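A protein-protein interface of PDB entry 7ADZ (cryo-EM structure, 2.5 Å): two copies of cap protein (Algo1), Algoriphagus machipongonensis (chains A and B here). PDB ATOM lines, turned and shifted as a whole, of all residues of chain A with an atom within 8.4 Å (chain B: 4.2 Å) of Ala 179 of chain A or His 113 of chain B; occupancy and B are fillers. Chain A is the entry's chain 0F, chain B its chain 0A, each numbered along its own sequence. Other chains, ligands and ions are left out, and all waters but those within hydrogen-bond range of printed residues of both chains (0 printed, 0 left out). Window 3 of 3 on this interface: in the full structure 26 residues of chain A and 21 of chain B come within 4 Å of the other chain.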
ATOM      1  N   ASN A  67     -12.540 -14.584 -17.302  1.00  0.00           N
ATOM      2  CA  ASN A  67     -13.872 -14.839 -16.759  1.00  0.00           C
ATOM      3  C   ASN A  67     -14.981 -14.726 -17.812  1.00  0.00           C
ATOM      4  O   ASN A  67     -16.091 -14.302 -17.485  1.00  0.00           O
ATOM      5  CB  ASN A  67     -14.146 -13.882 -15.594  1.00  0.00           C
ATOM      6  CG  ASN A  67     -15.114 -14.449 -14.578  1.00  0.00           C
ATOM      7  OD1 ASN A  67     -15.330 -15.657 -14.514  1.00  0.00           O
ATOM      8  ND2 ASN A  67     -15.712 -13.574 -13.782  1.00  0.00           N
ATOM      9  N   THR A  76     -20.430 -13.647 -23.647  1.00  0.00           N
ATOM     10  CA  THR A  76     -20.611 -12.530 -22.724  1.00  0.00           C
ATOM     11  C   THR A  76     -19.291 -12.259 -22.013  1.00  0.00           C
ATOM     12  O   THR A  76     -18.616 -13.195 -21.579  1.00  0.00           O
ATOM     13  CB  THR A  76     -21.704 -12.814 -21.688  1.00  0.00           C
ATOM     14  OG1 THR A  76     -21.246 -13.807 -20.771  1.00  0.00           O
ATOM     15  CG2 THR A  76     -22.941 -13.337 -22.360  1.00  0.00           C
ATOM     16  N   TYR A  77     -18.938 -10.982 -21.882  1.00  0.00           N
ATOM     17  CA  TYR A  77     -17.665 -10.556 -21.309  1.00  0.00           C
ATOM     18  C   TYR A  77     -17.858 -10.068 -19.877  1.00  0.00           C
ATOM     19  O   TYR A  77     -18.795  -9.316 -19.597  1.00  0.00           O
ATOM     20  CB  TYR A  77     -17.050  -9.445 -22.154  1.00  0.00           C
ATOM     21  CG  TYR A  77     -16.585  -9.874 -23.520  1.00  0.00           C
ATOM     22  CD1 TYR A  77     -15.331 -10.435 -23.700  1.00  0.00           C
ATOM     23  CD2 TYR A  77     -17.396  -9.704 -24.636  1.00  0.00           C
ATOM     24  CE1 TYR A  77     -14.896 -10.825 -24.944  1.00  0.00           C
ATOM     25  CE2 TYR A  77     -16.970 -10.092 -25.889  1.00  0.00           C
ATOM     26  CZ  TYR A  77     -15.715 -10.652 -26.036  1.00  0.00           C
ATOM     27  OH  TYR A  77     -15.273 -11.042 -27.276  1.00  0.00           O
ATOM     28  N   LYS A  78     -16.980 -10.509 -18.969  1.00  0.00           N
ATOM     29  CA  LYS A  78     -16.992 -10.086 -17.571  1.00  0.00           C
ATOM     30  C   LYS A  78     -15.572  -9.772 -17.107  1.00  0.00           C
ATOM     31  O   LYS A  78     -14.592 -10.206 -17.714  1.00  0.00           O
ATOM     32  CB  LYS A  78     -17.587 -11.151 -16.627  1.00  0.00           C
ATOM     33  CG  LYS A  78     -18.754 -11.952 -17.162  1.00  0.00           C
ATOM     34  CD  LYS A  78     -19.595 -12.520 -16.052  1.00  0.00           C
ATOM     35  CE  LYS A  78     -20.728 -13.343 -16.610  1.00  0.00           C
ATOM     36  NZ  LYS A  78     -21.820 -13.527 -15.627  1.00  0.00           N
ATOM     37  N   ASN A  79     -15.471  -9.014 -15.999  1.00  0.00           N
ATOM     38  CA  ASN A  79     -14.191  -8.692 -15.376  1.00  0.00           C
ATOM     39  C   ASN A  79     -13.680  -9.862 -14.531  1.00  0.00           C
ATOM     40  O   ASN A  79     -14.473 -10.664 -14.035  1.00  0.00           O
ATOM     41  CB  ASN A  79     -14.320  -7.449 -14.501  1.00  0.00           C
ATOM     42  CG  ASN A  79     -14.646  -6.212 -15.294  1.00  0.00           C
ATOM     43  OD1 ASN A  79     -13.869  -5.781 -16.138  1.00  0.00           O
ATOM     44  ND2 ASN A  79     -15.802  -5.629 -15.027  1.00  0.00           N
ATOM     45  N   PRO A  80     -12.359  -9.991 -14.369  1.00  0.00           N
ATOM     46  CA  PRO A  80     -11.815 -11.059 -13.517  1.00  0.00           C
ATOM     47  C   PRO A  80     -12.125 -10.853 -12.039  1.00  0.00           C
ATOM     48  O   PRO A  80     -12.201  -9.727 -11.547  1.00  0.00           O
ATOM     49  CB  PRO A  80     -10.308 -10.992 -13.781  1.00  0.00           C
ATOM     50  CG  PRO A  80     -10.170 -10.295 -15.075  1.00  0.00           C
ATOM     51  CD  PRO A  80     -11.298  -9.330 -15.151  1.00  0.00           C
ATOM     52  N   LEU A  82     -11.500 -11.028  -7.989  1.00  0.00           N
ATOM     53  CA  LEU A  82     -10.630 -10.505  -6.943  1.00  0.00           C
ATOM     54  C   LEU A  82     -10.386 -11.588  -5.893  1.00  0.00           C
ATOM     55  O   LEU A  82     -11.335 -12.161  -5.357  1.00  0.00           O
ATOM     56  CB  LEU A  82     -11.320  -9.285  -6.310  1.00  0.00           C
ATOM     57  CG  LEU A  82     -10.667  -8.341  -5.295  1.00  0.00           C
ATOM     58  CD1 LEU A  82      -9.152  -8.380  -5.420  1.00  0.00           C
ATOM     59  CD2 LEU A  82     -11.186  -6.922  -5.469  1.00  0.00           C
ATOM     60  N   ILE A 175     -14.442 -12.239  -4.072  1.00  0.00           N
ATOM     61  CA  ILE A 175     -15.211 -11.007  -4.239  1.00  0.00           C
ATOM     62  C   ILE A 175     -15.413 -10.771  -5.732  1.00  0.00           C
ATOM     63  O   ILE A 175     -14.438 -10.674  -6.487  1.00  0.00           O
ATOM     64  CB  ILE A 175     -14.508  -9.812  -3.578  1.00  0.00           C
ATOM     65  CG1 ILE A 175     -14.555  -9.950  -2.058  1.00  0.00           C
ATOM     66  CG2 ILE A 175     -15.132  -8.496  -4.019  1.00  0.00           C
ATOM     67  CD1 ILE A 175     -13.876  -8.832  -1.330  1.00  0.00           C
ATOM     68  N   ASP A 176     -16.673 -10.664  -6.153  1.00  0.00           N
ATOM     69  CA  ASP A 176     -16.999 -10.595  -7.577  1.00  0.00           C
ATOM     70  C   ASP A 176     -18.406 -10.047  -7.743  1.00  0.00           C
ATOM     71  O   ASP A 176     -19.346 -10.565  -7.137  1.00  0.00           O
ATOM     72  CB  ASP A 176     -16.867 -11.978  -8.218  1.00  0.00           C
ATOM     73  CG  ASP A 176     -17.367 -12.016  -9.639  1.00  0.00           C
ATOM     74  OD1 ASP A 176     -18.353 -12.733  -9.895  1.00  0.00           O
ATOM     75  OD2 ASP A 176     -16.788 -11.323 -10.498  1.00  0.00           O
ATOM     76  N   ARG A 177     -18.551  -9.004  -8.563  1.00  0.00           N
ATOM     77  CA  ARG A 177     -19.860  -8.394  -8.785  1.00  0.00           C
ATOM     78  C   ARG A 177     -20.677  -9.180  -9.806  1.00  0.00           C
ATOM     79  O   ARG A 177     -21.914  -9.134  -9.781  1.00  0.00           O
ATOM     80  CB  ARG A 177     -19.678  -6.946  -9.236  1.00  0.00           C
ATOM     81  CG  ARG A 177     -20.943  -6.113  -9.258  1.00  0.00           C
ATOM     82  CD  ARG A 177     -20.707  -4.753  -8.652  1.00  0.00           C
ATOM     83  NE  ARG A 177     -21.886  -3.905  -8.763  1.00  0.00           N
ATOM     84  CZ  ARG A 177     -21.978  -2.689  -8.247  1.00  0.00           C
ATOM     85  NH1 ARG A 177     -23.088  -1.988  -8.397  1.00  0.00           N
ATOM     86  NH2 ARG A 177     -20.955  -2.174  -7.585  1.00  0.00           N
ATOM     87  N   ASP A 178     -19.992  -9.880 -10.722  1.00  0.00           N
ATOM     88  CA  ASP A 178     -20.574 -10.772 -11.730  1.00  0.00           C
ATOM     89  C   ASP A 178     -21.463 -10.012 -12.721  1.00  0.00           C
ATOM     90  O   ASP A 178     -22.523 -10.496 -13.120  1.00  0.00           O
ATOM     91  CB  ASP A 178     -21.333 -11.939 -11.073  1.00  0.00           C
ATOM     92  CG  ASP A 178     -21.451 -13.155 -11.966  1.00  0.00           C
ATOM     93  OD1 ASP A 178     -20.950 -13.114 -13.104  1.00  0.00           O
ATOM     94  OD2 ASP A 178     -22.038 -14.162 -11.520  1.00  0.00           O
ATOM     95  N   ALA A 179     -21.042  -8.813 -13.119  1.00  0.00           N
ATOM     96  CA  ALA A 179     -21.806  -7.991 -14.046  1.00  0.00           C
ATOM     97  C   ALA A 179     -21.300  -8.140 -15.479  1.00  0.00           C
ATOM     98  O   ALA A 179     -20.132  -8.449 -15.721  1.00  0.00           O
ATOM     99  CB  ALA A 179     -21.752  -6.523 -13.627  1.00  0.00           C
ATOM    100  N   THR A 180     -22.198  -7.894 -16.430  1.00  0.00           N
ATOM    101  CA  THR A 180     -21.928  -8.069 -17.854  1.00  0.00           C
ATOM    102  C   THR A 180     -21.456  -6.747 -18.451  1.00  0.00           C
ATOM    103  O   THR A 180     -22.033  -5.695 -18.166  1.00  0.00           O
ATOM    104  CB  THR A 180     -23.187  -8.572 -18.566  1.00  0.00           C
ATOM    105  OG1 THR A 180     -23.561  -9.838 -18.020  1.00  0.00           O
ATOM    106  CG2 THR A 180     -22.959  -8.736 -20.052  1.00  0.00           C
ATOM    107  N   THR A 181     -20.387  -6.796 -19.253  1.00  0.00           N
ATOM    108  CA  THR A 181     -19.933  -5.593 -19.942  1.00  0.00           C
ATOM    109  C   THR A 181     -20.357  -5.580 -21.411  1.00  0.00           C
ATOM    110  O   THR A 181     -20.629  -4.511 -21.963  1.00  0.00           O
ATOM    111  CB  THR A 181     -18.415  -5.445 -19.827  1.00  0.00           C
ATOM    112  OG1 THR A 181     -17.771  -6.261 -20.812  1.00  0.00           O
ATOM    113  CG2 THR A 181     -17.937  -5.860 -18.450  1.00  0.00           C
ATOM    114  N   SER A 182     -20.424  -6.744 -22.060  1.00  0.00           N
ATOM    115  CA  SER A 182     -20.653  -6.789 -23.500  1.00  0.00           C
ATOM    116  C   SER A 182     -21.171  -8.161 -23.911  1.00  0.00           C
ATOM    117  O   SER A 182     -21.004  -9.148 -23.192  1.00  0.00           O
ATOM    118  CB  SER A 182     -19.368  -6.457 -24.268  1.00  0.00           C
ATOM    119  OG  SER A 182     -19.565  -6.525 -25.666  1.00  0.00           O
ATOM    120  N   GLU B 109     -16.072  -4.168  -3.952  1.00  0.00           N
ATOM    121  CA  GLU B 109     -16.860  -4.676  -5.071  1.00  0.00           C
ATOM    122  C   GLU B 109     -17.021  -3.620  -6.159  1.00  0.00           C
ATOM    123  O   GLU B 109     -17.071  -3.949  -7.347  1.00  0.00           O
ATOM    124  CB  GLU B 109     -18.227  -5.143  -4.571  1.00  0.00           C
ATOM    125  CG  GLU B 109     -19.050  -5.915  -5.578  1.00  0.00           C
ATOM    126  CD  GLU B 109     -20.451  -6.223  -5.076  1.00  0.00           C
ATOM    127  OE1 GLU B 109     -20.821  -5.731  -3.991  1.00  0.00           O
ATOM    128  OE2 GLU B 109     -21.181  -6.973  -5.758  1.00  0.00           O
ATOM    129  N   PHE B 110     -17.089  -2.345  -5.768  1.00  0.00           N
ATOM    130  CA  PHE B 110     -17.320  -1.265  -6.722  1.00  0.00           C
ATOM    131  C   PHE B 110     -16.109  -1.034  -7.620  1.00  0.00           C
ATOM    132  O   PHE B 110     -16.258  -0.841  -8.831  1.00  0.00           O
ATOM    133  CB  PHE B 110     -17.694   0.009  -5.964  1.00  0.00           C
ATOM    134  CG  PHE B 110     -17.786   1.232  -6.826  1.00  0.00           C
ATOM    135  CD1 PHE B 110     -18.819   1.379  -7.735  1.00  0.00           C
ATOM    136  CD2 PHE B 110     -16.847   2.243  -6.719  1.00  0.00           C
ATOM    137  CE1 PHE B 110     -18.903   2.498  -8.528  1.00  0.00           C
ATOM    138  CE2 PHE B 110     -16.929   3.368  -7.508  1.00  0.00           C
ATOM    139  CZ  PHE B 110     -17.958   3.496  -8.413  1.00  0.00           C
ATOM    140  N   PHE B 111     -14.902  -1.065  -7.056  1.00  0.00           N
ATOM    141  CA  PHE B 111     -13.718  -0.797  -7.867  1.00  0.00           C
ATOM    142  C   PHE B 111     -13.269  -2.031  -8.631  1.00  0.00           C
ATOM    143  O   PHE B 111     -12.458  -1.921  -9.556  1.00  0.00           O
ATOM    144  CB  PHE B 111     -12.587  -0.246  -6.998  1.00  0.00           C
ATOM    145  CG  PHE B 111     -12.803   1.175  -6.578  1.00  0.00           C
ATOM    146  CD1 PHE B 111     -12.863   2.184  -7.523  1.00  0.00           C
ATOM    147  CD2 PHE B 111     -12.974   1.500  -5.244  1.00  0.00           C
ATOM    148  CE1 PHE B 111     -13.078   3.489  -7.142  1.00  0.00           C
ATOM    149  CE2 PHE B 111     -13.186   2.802  -4.857  1.00  0.00           C
ATOM    150  CZ  PHE B 111     -13.241   3.797  -5.806  1.00  0.00           C
ATOM    151  N   GLN B 112     -13.784  -3.207  -8.267  1.00  0.00           N
ATOM    152  CA  GLN B 112     -13.550  -4.404  -9.067  1.00  0.00           C
ATOM    153  C   GLN B 112     -14.248  -4.304 -10.421  1.00  0.00           C
ATOM    154  O   GLN B 112     -13.760  -4.839 -11.422  1.00  0.00           O
ATOM    155  CB  GLN B 112     -14.017  -5.638  -8.292  1.00  0.00           C
ATOM    156  CG  GLN B 112     -13.742  -6.976  -8.956  1.00  0.00           C
ATOM    157  CD  GLN B 112     -14.964  -7.548  -9.649  1.00  0.00           C
ATOM    158  OE1 GLN B 112     -16.085  -7.112  -9.409  1.00  0.00           O
ATOM    159  NE2 GLN B 112     -14.747  -8.520 -10.517  1.00  0.00           N
ATOM    160  N   HIS B 113     -15.367  -3.581 -10.479  1.00  0.00           N
ATOM    161  CA  HIS B 113     -16.170  -3.529 -11.695  1.00  0.00           C
ATOM    162  C   HIS B 113     -15.837  -2.313 -12.559  1.00  0.00           C
ATOM    163  O   HIS B 113     -15.866  -2.402 -13.791  1.00  0.00           O
ATOM    164  CB  HIS B 113     -17.650  -3.560 -11.319  1.00  0.00           C
ATOM    165  CG  HIS B 113     -18.576  -3.586 -12.491  1.00  0.00           C
ATOM    166  ND1 HIS B 113     -19.202  -2.456 -12.971  1.00  0.00           N
ATOM    167  CD2 HIS B 113     -18.956  -4.599 -13.306  1.00  0.00           C
ATOM    168  CE1 HIS B 113     -19.949  -2.777 -14.012  1.00  0.00           C
ATOM    169  NE2 HIS B 113     -19.812  -4.071 -14.240  1.00  0.00           N
ATOM    170  N   LYS B 114     -15.511  -1.178 -11.946  1.00  0.00           N
ATOM    171  CA  LYS B 114     -15.252   0.062 -12.677  1.00  0.00           C
ATOM    172  C   LYS B 114     -13.941   0.662 -12.193  1.00  0.00           C
ATOM    173  O   LYS B 114     -13.818   1.006 -11.015  1.00  0.00           O
ATOM    174  CB  LYS B 114     -16.399   1.058 -12.483  1.00  0.00           C
ATOM    175  CG  LYS B 114     -16.306   2.309 -13.338  1.00  0.00           C
ATOM    176  CD  LYS B 114     -17.327   3.342 -12.895  1.00  0.00           C
ATOM    177  CE  LYS B 114     -17.572   4.395 -13.963  1.00  0.00           C
ATOM    178  NZ  LYS B 114     -16.316   4.961 -14.512  1.00  0.00           N
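The side-chain amide nitrogen of Gln 112 of chain B is in hydrogen-bond range of the backbone carbonyl oxygen of Pro 80 of chain A (3.0 Å). The side-chain amide nitrogen (NE2) of Gln 112 of chain B is in hydrogen-bond range of the side-chain carboxylate (OD2) of Asp 176 of chain A, at 3.5 Å. The side-chain amide oxygen (OE1) of Gln 112 of chain B is in hydrogen-bond range of the backbone NH (N) of Arg 177 of chain A. The backbone carbonyl oxygen (O) of His 113 of chain B lies within hydrogen-bond range of the side-chain amide nitrogen (ND2) of Asn 79 of chain A (3.5 Å).
The side-chain amide nitrogen of Asn 67 of chain A is in hydrogen-bond range of the backbone carbonyl oxygen of Asn 79 of chain A. OD1 of Asp 176 of chain A sits close to N of Asp 178 of chain A, 3.4 Å away.
Glu 109 of chain B touches Arg 177 of chain A (OE2 to CA, 3.6 Å). NH2 of Arg 177 of chain A touches CA of Phe 110 of chain B (3.8 Å). Ala 179 of chain A touches His 113 of chain B.
Of the printed residues of chain B, Asn 79 of chain A touches His 113. Printed residues of chain B within 4 Å of Pro 80 of chain A: Gln 112 (3.0 Å). Of the printed residues of chain B, Arg 177 of chain A touches Glu 109, Phe 110 and Gln 112. Ala 179 of chain A touches one residue of chain B. Printed residues of chain A within 4 Å of Phe 110 of chain B: Arg 177. Of the printed residues of chain A, Gln 112 of chain B touches Pro 80, Asp 176 and Arg 177. Of chain A, only Asn 79 and Ala 179 come within 4 Å of His 113 of chain B. The nearest printed residue of chain B that does not touch Ala 179 of chain A is Gln 112 of chain B (6.4 Å).
Of the 6 printed residues of chain B, 4 touch a printed residue of chain A. Hydrophobic or aromatic side chains of chain B that line the printed part of chain A: His 113. Hydrophobic or aromatic side chains of chain A within 4 Å of the printed part of chain B: Ala 179.
No position is printed for both chains.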
